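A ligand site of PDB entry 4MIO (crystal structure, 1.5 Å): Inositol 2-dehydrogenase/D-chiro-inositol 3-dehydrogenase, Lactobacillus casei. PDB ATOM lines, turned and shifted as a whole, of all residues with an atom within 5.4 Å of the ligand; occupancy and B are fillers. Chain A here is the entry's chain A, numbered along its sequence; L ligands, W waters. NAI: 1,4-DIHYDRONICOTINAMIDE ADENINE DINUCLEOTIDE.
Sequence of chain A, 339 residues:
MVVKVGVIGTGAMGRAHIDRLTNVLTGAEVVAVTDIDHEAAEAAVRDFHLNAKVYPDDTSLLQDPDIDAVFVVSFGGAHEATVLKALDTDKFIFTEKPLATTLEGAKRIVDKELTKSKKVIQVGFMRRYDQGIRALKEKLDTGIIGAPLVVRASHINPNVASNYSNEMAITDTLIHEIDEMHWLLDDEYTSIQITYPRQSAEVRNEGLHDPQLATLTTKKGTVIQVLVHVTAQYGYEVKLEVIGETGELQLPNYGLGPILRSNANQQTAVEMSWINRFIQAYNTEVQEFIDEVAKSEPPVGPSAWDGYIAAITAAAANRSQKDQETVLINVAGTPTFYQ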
ATOM      1  N   ILE A   8     -25.793 -15.976 -30.953  1.00  0.00           N
ATOM      2  CA  ILE A   8     -26.072 -15.503 -29.617  1.00  0.00           C
ATOM      3  C   ILE A   8     -25.935 -16.682 -28.619  1.00  0.00           C
ATOM      4  O   ILE A   8     -26.778 -17.532 -28.542  1.00  0.00           O
ATOM      5  CB  ILE A   8     -27.453 -14.911 -29.523  1.00  0.00           C
ATOM      6  CG1 ILE A   8     -27.636 -13.750 -30.510  1.00  0.00           C
ATOM      7  CG2 ILE A   8     -27.760 -14.499 -28.104  1.00  0.00           C
ATOM      8  CD1 ILE A   8     -29.001 -13.354 -30.737  1.00  0.00           C
ATOM      9  N   GLY A   9     -24.855 -16.651 -27.865  1.00  0.00           N
ATOM     10  CA  GLY A   9     -24.485 -17.702 -26.955  1.00  0.00           C
ATOM     11  C   GLY A   9     -23.420 -18.561 -27.574  1.00  0.00           C
ATOM     12  O   GLY A   9     -23.714 -19.340 -28.459  1.00  0.00           O
ATOM     13  N   THR A  10     -22.194 -18.419 -27.127  1.00  0.00           N
ATOM     14  CA  THR A  10     -21.080 -19.144 -27.673  1.00  0.00           C
ATOM     15  C   THR A  10     -20.449 -20.118 -26.670  1.00  0.00           C
ATOM     16  O   THR A  10     -19.266 -20.088 -26.428  1.00  0.00           O
ATOM     17  CB  THR A  10     -20.015 -18.202 -28.248  1.00  0.00           C
ATOM     18  OG1 THR A  10     -19.432 -17.435 -27.207  1.00  0.00           O
ATOM     19  CG2 THR A  10     -20.651 -17.246 -29.250  1.00  0.00           C
ATOM     20  N   GLY A  11     -21.294 -20.978 -26.132  1.00  0.00           N
ATOM     21  CA  GLY A  11     -20.892 -22.028 -25.233  1.00  0.00           C
ATOM     22  C   GLY A  11     -20.633 -23.311 -25.963  1.00  0.00           C
ATOM     23  O   GLY A  11     -20.145 -23.268 -27.033  1.00  0.00           O
ATOM     24  N   ALA A  12     -20.948 -24.430 -25.331  1.00  0.00           N
ATOM     25  CA  ALA A  12     -20.723 -25.728 -25.931  1.00  0.00           C
ATOM     26  C   ALA A  12     -21.421 -25.905 -27.295  1.00  0.00           C
ATOM     27  O   ALA A  12     -20.770 -26.206 -28.263  1.00  0.00           O
ATOM     28  CB  ALA A  12     -21.153 -26.852 -24.957  1.00  0.00           C
ATOM     29  N   MET A  13     -22.726 -25.745 -27.314  1.00  0.00           N
ATOM     30  CA  MET A  13     -23.508 -25.965 -28.535  1.00  0.00           C
ATOM     31  C   MET A  13     -23.349 -24.807 -29.506  1.00  0.00           C
ATOM     32  O   MET A  13     -23.340 -24.988 -30.680  1.00  0.00           O
ATOM     33  CB  MET A  13     -24.953 -26.228 -28.193  1.00  0.00           C
ATOM     34  CG  MET A  13     -25.807 -26.704 -29.322  1.00  0.00           C
ATOM     35  SD  MET A  13     -25.109 -28.163 -30.082  1.00  0.00           S
ATOM     36  CE  MET A  13     -26.570 -28.915 -30.751  1.00  0.00           C
ATOM     37  N   GLY A  14     -23.186 -23.610 -28.948  1.00  0.00           N
ATOM     38  CA  GLY A  14     -22.901 -22.448 -29.751  1.00  0.00           C
ATOM     39  C   GLY A  14     -21.652 -22.619 -30.552  1.00  0.00           C
ATOM     40  O   GLY A  14     -21.639 -22.343 -31.715  1.00  0.00           O
ATOM     41  N   THR A  34     -22.216 -12.887 -29.791  1.00  0.00           N
ATOM     42  CA  THR A  34     -22.411 -12.263 -28.493  1.00  0.00           C
ATOM     43  C   THR A  34     -22.604 -13.323 -27.395  1.00  0.00           C
ATOM     44  O   THR A  34     -23.165 -14.351 -27.634  1.00  0.00           O
ATOM     45  CB  THR A  34     -23.578 -11.246 -28.479  1.00  0.00           C
ATOM     46  OG1 THR A  34     -23.543 -10.503 -27.259  1.00  0.00           O
ATOM     47  CG2 THR A  34     -24.887 -11.870 -28.595  1.00  0.00           C
ATOM     48  N   ASP A  35     -22.150 -13.011 -26.193  1.00  0.00           N
ATOM     49  CA  ASP A  35     -22.271 -13.892 -25.043  1.00  0.00           C
ATOM     50  C   ASP A  35     -22.187 -13.015 -23.770  1.00  0.00           C
ATOM     51  O   ASP A  35     -21.471 -12.063 -23.790  1.00  0.00           O
ATOM     52  CB  ASP A  35     -21.148 -14.918 -25.076  1.00  0.00           C
ATOM     53  CG  ASP A  35     -21.383 -16.088 -24.153  1.00  0.00           C
ATOM     54  OD1 ASP A  35     -21.364 -15.882 -22.941  1.00  0.00           O
ATOM     55  OD2 ASP A  35     -21.625 -17.197 -24.634  1.00  0.00           O
ATOM     56  N   ILE A  36     -22.934 -13.349 -22.744  1.00  0.00           N
ATOM     57  CA  ILE A  36     -22.847 -12.609 -21.485  1.00  0.00           C
ATOM     58  C   ILE A  36     -21.480 -12.741 -20.928  1.00  0.00           C
ATOM     59  O   ILE A  36     -21.022 -11.899 -20.159  1.00  0.00           O
ATOM     60  CB  ILE A  36     -23.889 -13.069 -20.471  1.00  0.00           C
ATOM     61  CG1 ILE A  36     -23.736 -14.553 -20.140  1.00  0.00           C
ATOM     62  CG2 ILE A  36     -25.238 -12.763 -20.955  1.00  0.00           C
ATOM     63  CD1 ILE A  36     -24.731 -15.029 -19.176  1.00  0.00           C
ATOM     64  N   ASP A  37     -20.802 -13.793 -21.324  1.00  0.00           N
ATOM     65  CA  ASP A  37     -19.434 -13.958 -21.036  1.00  0.00           C
ATOM     66  C   ASP A  37     -18.593 -13.510 -22.178  1.00  0.00           C
ATOM     67  O   ASP A  37     -18.192 -14.254 -23.013  1.00  0.00           O
ATOM     68  CB  ASP A  37     -19.134 -15.398 -20.650  1.00  0.00           C
ATOM     69  CG  ASP A  37     -17.709 -15.618 -20.290  1.00  0.00           C
ATOM     70  OD1 ASP A  37     -16.895 -14.722 -20.459  1.00  0.00           O
ATOM     71  OD2 ASP A  37     -17.361 -16.705 -19.849  1.00  0.00           O
ATOM     72  N   ALA A  40     -15.951 -15.549 -23.621  1.00  0.00           N
ATOM     73  CA  ALA A  40     -16.358 -16.689 -24.438  1.00  0.00           C
ATOM     74  C   ALA A  40     -16.578 -16.245 -25.865  1.00  0.00           C
ATOM     75  O   ALA A  40     -16.201 -16.923 -26.773  1.00  0.00           O
ATOM     76  CB  ALA A  40     -17.572 -17.350 -23.893  1.00  0.00           C
ATOM     77  N   VAL A  73     -28.354 -19.720 -29.029  1.00  0.00           N
ATOM     78  CA  VAL A  73     -27.749 -20.859 -28.369  1.00  0.00           C
ATOM     79  C   VAL A  73     -27.304 -20.545 -26.927  1.00  0.00           C
ATOM     80  O   VAL A  73     -26.375 -21.086 -26.437  1.00  0.00           O
ATOM     81  CB  VAL A  73     -26.556 -21.410 -29.173  1.00  0.00           C
ATOM     82  CG1 VAL A  73     -26.448 -22.908 -28.972  1.00  0.00           C
ATOM     83  CG2 VAL A  73     -26.730 -21.096 -30.645  1.00  0.00           C
ATOM     84  N   SER A  74     -28.068 -19.686 -26.301  1.00  0.00           N
ATOM     85  CA  SER A  74     -27.854 -19.309 -24.919  1.00  0.00           C
ATOM     86  C   SER A  74     -28.545 -20.288 -23.977  1.00  0.00           C
ATOM     87  O   SER A  74     -29.069 -21.293 -24.408  1.00  0.00           O
ATOM     88  CB  SER A  74     -28.370 -17.897 -24.740  1.00  0.00           C
ATOM     89  OG  SER A  74     -29.686 -17.772 -25.128  1.00  0.00           O
ATOM     90  N   PHE A  75     -28.534 -20.003 -22.678  1.00  0.00           N
ATOM     91  CA  PHE A  75     -29.284 -20.787 -21.724  1.00  0.00           C
ATOM     92  C   PHE A  75     -30.727 -20.889 -22.180  1.00  0.00           C
ATOM     93  O   PHE A  75     -31.266 -19.962 -22.732  1.00  0.00           O
ATOM     94  CB  PHE A  75     -29.264 -20.177 -20.308  1.00  0.00           C
ATOM     95  CG  PHE A  75     -27.909 -20.093 -19.670  1.00  0.00           C
ATOM     96  CD1 PHE A  75     -26.925 -20.949 -20.008  1.00  0.00           C
ATOM     97  CD2 PHE A  75     -27.640 -19.148 -18.712  1.00  0.00           C
ATOM     98  CE1 PHE A  75     -25.694 -20.864 -19.429  1.00  0.00           C
ATOM     99  CE2 PHE A  75     -26.400 -19.066 -18.143  1.00  0.00           C
ATOM    100  CZ  PHE A  75     -25.445 -19.913 -18.481  1.00  0.00           C
ATOM    101  N   GLY A  76     -31.348 -22.024 -21.934  1.00  0.00           N
ATOM    102  CA  GLY A  76     -32.689 -22.205 -22.358  1.00  0.00           C
ATOM    103  C   GLY A  76     -33.628 -21.119 -21.910  1.00  0.00           C
ATOM    104  O   GLY A  76     -34.473 -20.684 -22.627  1.00  0.00           O
ATOM    105  N   ALA A  78     -33.121 -18.186 -21.529  1.00  0.00           N
ATOM    106  CA  ALA A  78     -32.809 -16.932 -22.196  1.00  0.00           C
ATOM    107  C   ALA A  78     -33.310 -16.856 -23.634  1.00  0.00           C
ATOM    108  O   ALA A  78     -33.159 -15.836 -24.259  1.00  0.00           O
ATOM    109  CB  ALA A  78     -31.361 -16.663 -22.158  1.00  0.00           C
ATOM    110  N   HIS A  79     -33.912 -17.916 -24.142  1.00  0.00           N
ATOM    111  CA  HIS A  79     -34.341 -17.952 -25.525  1.00  0.00           C
ATOM    112  C   HIS A  79     -35.533 -17.056 -25.797  1.00  0.00           C
ATOM    113  O   HIS A  79     -35.536 -16.360 -26.757  1.00  0.00           O
ATOM    114  CB  HIS A  79     -34.634 -19.388 -25.982  1.00  0.00           C
ATOM    115  CG  HIS A  79     -33.433 -20.288 -25.971  1.00  0.00           C
ATOM    116  ND1 HIS A  79     -33.503 -21.598 -26.376  1.00  0.00           N
ATOM    117  CD2 HIS A  79     -32.148 -20.083 -25.607  1.00  0.00           C
ATOM    118  CE1 HIS A  79     -32.314 -22.137 -26.290  1.00  0.00           C
ATOM    119  NE2 HIS A  79     -31.480 -21.248 -25.808  1.00  0.00           N
ATOM    120  N   THR A  82     -34.821 -13.321 -26.173  1.00  0.00           N
ATOM    121  CA  THR A  82     -34.014 -13.104 -27.354  1.00  0.00           C
ATOM    122  C   THR A  82     -34.803 -13.346 -28.645  1.00  0.00           C
ATOM    123  O   THR A  82     -34.682 -12.581 -29.579  1.00  0.00           O
ATOM    124  CB  THR A  82     -32.732 -13.934 -27.348  1.00  0.00           C
ATOM    125  OG1 THR A  82     -31.907 -13.525 -26.275  1.00  0.00           O
ATOM    126  CG2 THR A  82     -31.947 -13.756 -28.617  1.00  0.00           C
ATOM    127  N   GLU A  96     -32.031 -23.012 -30.701  1.00  0.00           N
ATOM    128  CA  GLU A  96     -31.948 -24.307 -30.078  1.00  0.00           C
ATOM    129  C   GLU A  96     -33.185 -24.533 -29.230  1.00  0.00           C
ATOM    130  O   GLU A  96     -33.829 -23.615 -28.839  1.00  0.00           O
ATOM    131  CB  GLU A  96     -30.659 -24.458 -29.269  1.00  0.00           C
ATOM    132  CG  GLU A  96     -29.503 -25.068 -30.020  1.00  0.00           C
ATOM    133  CD  GLU A  96     -29.834 -26.417 -30.629  1.00  0.00           C
ATOM    134  OE1 GLU A  96     -30.798 -27.040 -30.180  1.00  0.00           O
ATOM    135  OE2 GLU A  96     -29.132 -26.833 -31.523  1.00  0.00           O
ATOM    136  N   LYS A  97     -33.502 -25.805 -28.982  1.00  0.00           N
ATOM    137  CA  LYS A  97     -34.497 -26.134 -27.984  1.00  0.00           C
ATOM    138  C   LYS A  97     -34.030 -25.631 -26.620  1.00  0.00           C
ATOM    139  O   LYS A  97     -32.868 -25.532 -26.380  1.00  0.00           O
ATOM    140  CB  LYS A  97     -34.766 -27.637 -27.947  1.00  0.00           C
ATOM    141  CG  LYS A  97     -33.540 -28.450 -27.920  1.00  0.00           C
ATOM    142  CD  LYS A  97     -33.434 -29.406 -26.791  1.00  0.00           C
ATOM    143  CE  LYS A  97     -33.397 -28.732 -25.468  1.00  0.00           C
ATOM    144  NZ  LYS A  97     -32.535 -29.367 -24.482  1.00  0.00           N
ATOM    145  N   PRO A  98     -34.973 -25.262 -25.751  1.00  0.00           N
ATOM    146  CA  PRO A  98     -36.392 -25.133 -26.007  1.00  0.00           C
ATOM    147  C   PRO A  98     -36.738 -23.777 -26.680  1.00  0.00           C
ATOM    148  O   PRO A  98     -35.925 -22.924 -26.667  1.00  0.00           O
ATOM    149  CB  PRO A  98     -36.959 -25.128 -24.608  1.00  0.00           C
ATOM    150  CG  PRO A  98     -35.956 -24.564 -23.835  1.00  0.00           C
ATOM    151  CD  PRO A  98     -34.669 -24.931 -24.368  1.00  0.00           C
ATOM    152  N   GLY A 124     -34.388 -26.152 -32.929  1.00  0.00           N
ATOM    153  CA  GLY A 124     -33.410 -27.215 -33.089  1.00  0.00           C
ATOM    154  C   GLY A 124     -33.727 -28.634 -32.644  1.00  0.00           C
ATOM    155  O   GLY A 124     -32.909 -29.274 -32.028  1.00  0.00           O
ATOM    156  N   MET A 126     -33.419 -31.838 -33.696  1.00  0.00           N
ATOM    157  CA  MET A 126     -32.679 -32.521 -34.739  1.00  0.00           C
ATOM    158  C   MET A 126     -33.112 -33.942 -35.063  1.00  0.00           C
ATOM    159  O   MET A 126     -32.747 -34.445 -36.068  1.00  0.00           O
ATOM    160  CB  MET A 126     -31.194 -32.491 -34.470  1.00  0.00           C
ATOM    161  CG  MET A 126     -30.707 -33.531 -33.503  1.00  0.00           C
ATOM    162  SD  MET A 126     -31.345 -33.337 -31.840  1.00  0.00           S
ATOM    163  CE  MET A 126     -30.684 -34.830 -31.066  1.00  0.00           C
ATOM    164  N   ASP A 172     -34.445 -31.962 -21.164  1.00  0.00           N
ATOM    165  CA  ASP A 172     -33.240 -32.139 -21.914  1.00  0.00           C
ATOM    166  C   ASP A 172     -33.228 -33.488 -22.679  1.00  0.00           C
ATOM    167  O   ASP A 172     -32.582 -33.623 -23.673  1.00  0.00           O
ATOM    168  CB  ASP A 172     -32.005 -32.042 -21.035  1.00  0.00           C
ATOM    169  CG  ASP A 172     -31.725 -30.612 -20.558  1.00  0.00           C
ATOM    170  OD1 ASP A 172     -32.548 -29.736 -20.813  1.00  0.00           O
ATOM    171  OD2 ASP A 172     -30.712 -30.380 -19.921  1.00  0.00           O
ATOM    172  N   HIS A 176     -36.861 -34.730 -26.770  1.00  0.00           N
ATOM    173  CA  HIS A 176     -36.627 -35.180 -28.126  1.00  0.00           C
ATOM    174  C   HIS A 176     -37.728 -36.131 -28.641  1.00  0.00           C
ATOM    175  O   HIS A 176     -38.192 -35.998 -29.731  1.00  0.00           O
ATOM    176  CB  HIS A 176     -35.235 -35.807 -28.229  1.00  0.00           C
ATOM    177  CG  HIS A 176     -34.135 -34.820 -28.056  1.00  0.00           C
ATOM    178  ND1 HIS A 176     -33.802 -33.929 -29.038  1.00  0.00           N
ATOM    179  CD2 HIS A 176     -33.320 -34.555 -27.017  1.00  0.00           C
ATOM    180  CE1 HIS A 176     -32.817 -33.168 -28.604  1.00  0.00           C
ATOM    181  NE2 HIS A 176     -32.505 -33.544 -27.391  1.00  0.00           N
ATOM    182  N   TRP A 274     -23.963 -39.024 -27.131  1.00  0.00           N
ATOM    183  CA  TRP A 274     -25.071 -38.454 -27.890  1.00  0.00           C
ATOM    184  C   TRP A 274     -24.592 -37.484 -28.948  1.00  0.00           C
ATOM    185  O   TRP A 274     -25.198 -37.340 -29.997  1.00  0.00           O
ATOM    186  CB  TRP A 274     -26.128 -37.824 -27.001  1.00  0.00           C
ATOM    187  CG  TRP A 274     -25.675 -36.706 -26.133  1.00  0.00           C
ATOM    188  CD1 TRP A 274     -25.287 -36.777 -24.854  1.00  0.00           C
ATOM    189  CD2 TRP A 274     -25.580 -35.335 -26.502  1.00  0.00           C
ATOM    190  NE1 TRP A 274     -24.941 -35.554 -24.400  1.00  0.00           N
ATOM    191  CE2 TRP A 274     -25.110 -34.637 -25.397  1.00  0.00           C
ATOM    192  CE3 TRP A 274     -25.789 -34.633 -27.680  1.00  0.00           C
ATOM    193  CZ2 TRP A 274     -24.882 -33.278 -25.427  1.00  0.00           C
ATOM    194  CZ3 TRP A 274     -25.566 -33.292 -27.699  1.00  0.00           C
ATOM    195  CH2 TRP A 274     -25.117 -32.629 -26.572  1.00  0.00           C
ATOM    196  N   TYR A 282     -27.552 -33.044 -36.790  1.00  0.00           N
ATOM    197  CA  TYR A 282     -27.218 -31.642 -36.603  1.00  0.00           C
ATOM    198  C   TYR A 282     -26.763 -30.977 -37.889  1.00  0.00           C
ATOM    199  O   TYR A 282     -27.185 -29.894 -38.198  1.00  0.00           O
ATOM    200  CB  TYR A 282     -26.167 -31.463 -35.515  1.00  0.00           C
ATOM    201  CG  TYR A 282     -26.600 -31.828 -34.122  1.00  0.00           C
ATOM    202  CD1 TYR A 282     -27.705 -31.292 -33.548  1.00  0.00           C
ATOM    203  CD2 TYR A 282     -25.858 -32.700 -33.375  1.00  0.00           C
ATOM    204  CE1 TYR A 282     -28.100 -31.632 -32.277  1.00  0.00           C
ATOM    205  CE2 TYR A 282     -26.227 -33.059 -32.134  1.00  0.00           C
ATOM    206  CZ  TYR A 282     -27.344 -32.530 -31.560  1.00  0.00           C
ATOM    207  OH  TYR A 282     -27.687 -32.907 -30.308  1.00  0.00           O
HETATM  208  PA  NAI L   1     -23.572 -23.665 -22.314  1.00  0.00           P
HETATM  209  O1A NAI L   1     -23.858 -23.253 -20.976  1.00  0.00           O
HETATM  210  O2A NAI L   1     -22.365 -24.281 -22.635  1.00  0.00           O
HETATM  211  O5B NAI L   1     -23.569 -22.397 -23.228  1.00  0.00           O
HETATM  212  C5B NAI L   1     -24.476 -21.378 -23.138  1.00  0.00           C
HETATM  213  C4B NAI L   1     -23.806 -20.032 -23.464  1.00  0.00           C
HETATM  214  O4B NAI L   1     -24.762 -19.003 -23.473  1.00  0.00           O
HETATM  215  C3B NAI L   1     -22.853 -19.575 -22.375  1.00  0.00           C
HETATM  216  O3B NAI L   1     -21.646 -19.235 -22.947  1.00  0.00           O
HETATM  217  C2B NAI L   1     -23.530 -18.408 -21.714  1.00  0.00           C
HETATM  218  O2B NAI L   1     -22.619 -17.505 -21.154  1.00  0.00           O
HETATM  219  C1B NAI L   1     -24.269 -17.814 -22.859  1.00  0.00           C
HETATM  220  N9A NAI L   1     -25.445 -17.089 -22.453  1.00  0.00           N
HETATM  221  C8A NAI L   1     -26.276 -17.351 -21.489  1.00  0.00           C
HETATM  222  N7A NAI L   1     -27.296 -16.511 -21.480  1.00  0.00           N
HETATM  223  C5A NAI L   1     -27.097 -15.655 -22.460  1.00  0.00           C
HETATM  224  C6A NAI L   1     -27.771 -14.503 -23.019  1.00  0.00           C
HETATM  225  N6A NAI L   1     -28.897 -14.007 -22.543  1.00  0.00           N
HETATM  226  N1A NAI L   1     -27.228 -13.935 -24.081  1.00  0.00           N
HETATM  227  C2A NAI L   1     -26.131 -14.352 -24.600  1.00  0.00           C
HETATM  228  N3A NAI L   1     -25.453 -15.375 -24.136  1.00  0.00           N
HETATM  229  C4A NAI L   1     -25.902 -16.054 -23.100  1.00  0.00           C
HETATM  230  O3  NAI L   1     -24.858 -24.497 -22.732  1.00  0.00           O
HETATM  231  PN  NAI L   1     -25.094 -25.325 -24.105  1.00  0.00           P
HETATM  232  O1N NAI L   1     -24.946 -26.749 -23.857  1.00  0.00           O
HETATM  233  O2N NAI L   1     -24.228 -24.826 -25.129  1.00  0.00           O
HETATM  234  O5D NAI L   1     -26.563 -25.186 -24.451  1.00  0.00           O
HETATM  235  C5D NAI L   1     -27.041 -24.040 -25.092  1.00  0.00           C
HETATM  236  C4D NAI L   1     -28.421 -24.289 -25.633  1.00  0.00           C
HETATM  237  O4D NAI L   1     -28.339 -25.352 -26.551  1.00  0.00           O
HETATM  238  C3D NAI L   1     -29.367 -24.774 -24.569  1.00  0.00           C
HETATM  239  O3D NAI L   1     -30.621 -24.247 -24.884  1.00  0.00           O
HETATM  240  C2D NAI L   1     -29.374 -26.268 -24.766  1.00  0.00           C
HETATM  241  O2D NAI L   1     -30.603 -26.724 -24.360  1.00  0.00           O
HETATM  242  C1D NAI L   1     -29.276 -26.354 -26.266  1.00  0.00           C
HETATM  243  N1N NAI L   1     -28.786 -27.666 -26.678  1.00  0.00           N
HETATM  244  C2N NAI L   1     -29.448 -28.423 -27.528  1.00  0.00           C
HETATM  245  C3N NAI L   1     -29.023 -29.673 -27.912  1.00  0.00           C
HETATM  246  C7N NAI L   1     -29.825 -30.521 -28.876  1.00  0.00           C
HETATM  247  O7N NAI L   1     -29.617 -31.694 -28.900  1.00  0.00           O
HETATM  248  N7N NAI L   1     -30.710 -29.931 -29.629  1.00  0.00           N
HETATM  249  C4N NAI L   1     -27.725 -30.195 -27.428  1.00  0.00           C
HETATM  250  C5N NAI L   1     -27.095 -29.261 -26.545  1.00  0.00           C
HETATM  251  C6N NAI L   1     -27.649 -28.061 -26.237  1.00  0.00           C
HETATM  252  O   HOH W   1     -29.663 -33.127 -26.638  1.00  0.00           O
HETATM  253  O   HOH W   2     -23.803 -22.281 -26.433  1.00  0.00           O
HETATM  254  O   HOH W   3     -27.585 -11.186 -24.852  1.00  0.00           O
HETATM  255  O   HOH W   4     -24.902 -11.323 -24.914  1.00  0.00           O
HETATM  256  O   HOH W   5     -30.336 -28.987 -32.827  1.00  0.00           O
HETATM  257  O   HOH W   6     -31.224 -26.076 -21.535  1.00  0.00           O
HETATM  258  O   HOH W   7     -29.853 -15.160 -25.455  1.00  0.00           O
HETATM  259  O   HOH W   8     -23.937 -29.056 -24.846  1.00  0.00           O
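OD2 of Asp 35 sits at hydrogen-bond distance from N of Thr 10. The backbone NH (N) of Asp 37 sits at hydrogen-bond distance from the side-chain carboxylate (OD1) of Asp 35, 2.7 Å away. The backbone carbonyl oxygen of Glu 96 lies within hydrogen-bond range of a ring nitrogen (ND1) of His 79 (3.2 Å). The side-chain amino group of Lys 97 is in salt-bridge range of the side-chain carboxylate of Asp 172. A ring nitrogen (NE2) of His 79 sits close to the backbone carbonyl oxygen of Phe 75. O of Ile 8 lies within hydrogen-bond range of N of Val 73 (2.7 Å). The backbone carbonyl oxygen (O) of Ala 78 sits at hydrogen-bond distance from the side-chain hydroxyl (OG1) of Thr 82, 3.3 Å away. The backbone carbonyl oxygen (O) of Thr 34 is in hydrogen-bond range of the backbone NH (N) of Gly 9, 2.9 Å away.
The side-chain sulfur of Met 126 lies close to an oxygen (O7N) of the ligand (3.8 Å). Ile 8 touches the ligand. CA of Gly 9 touches O4B of the ligand, 3.7 Å away. Gly 11 touches the ligand. Ile 36 touches the ligand. Val 73 touches the ligand (O to C5D, 3.3 Å). Phe 75 touches the ligand (CE1 to O1A, 3.4 Å). N of Gly 76 touches O3D of the ligand (3.8 Å). CB of Ala 78 touches N6A of the ligand, 3.6 Å away. CE1 of His 176 touches O7N of the ligand, 3.5 Å away. Trp 274 touches the ligand (CH2 to C4N, 3.7 Å). Hydrophobic or aromatic side chains that line the ligand: Ile 8, Ala 12, Met 13, Ile 36, Val 73, Phe 75, Ala 78, His 79, Met 126, His 176, Trp 274 and Tyr 282.
Water W1 bridges an oxygen (O7N) of the ligand (2.7 Å) and a ring nitrogen (NE2) of His 176 (3.0 Å). Water W2 lies within hydrogen-bond range of the backbone carbonyl oxygen (O) of Val 73 (2.8 Å), the backbone NH (N) of Gly 11 (2.8 Å), an oxygen (O2N) of the ligand (2.9 Å) and the backbone NH (N) of Gly 14 (2.9 Å). Water W7 lies within hydrogen-bond range of the side-chain hydroxyl of Ser 74 (2.6 Å), the side-chain hydroxyl of Thr 82 (2.8 Å) and a nitrogen (N1A) of the ligand (3.2 Å). Water W4 lies within hydrogen-bond range of the side-chain hydroxyl of Thr 34 (2.8 Å) and the backbone NH of Asp 35 (3.5 Å). Water W5 lies within hydrogen-bond range of O of Gly 124, OE2 of Glu 96 and N7N of the ligand.
OD2 of Asp 35 lies within hydrogen-bond range of O3B of the ligand (2.6 Å). The side-chain hydroxyl of Tyr 282 is in hydrogen-bond range of an oxygen (O7N) of the ligand (2.7 Å). The backbone NH (N) of Met 13 lies within hydrogen-bond range of an oxygen (O2N) of the ligand (2.8 Å). N7N of the ligand lies within hydrogen-bond range of OE1 of Glu 96, 2.9 Å away. An oxygen (O3D) of the ligand sits at hydrogen-bond distance from the backbone carbonyl oxygen (O) of Lys 97 (3.0 Å). The side-chain amino group (NZ) of Lys 97 is in hydrogen-bond range of an oxygen (O2D) of the ligand (3.3 Å). A ring nitrogen (NE2) of His 79 lies close to an oxygen (O3D) of the ligand, 3.3 Å away. The backbone NH of Ala 12 lies within hydrogen-bond range of an oxygen (O2A) of the ligand, 3.0 Å away. An oxygen (O3D) of the ligand lies close to the backbone carbonyl oxygen of Ser 74 (3.4 Å). O of Gly 124 is in hydrogen-bond range of N7N of the ligand, 3.3 Å away.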
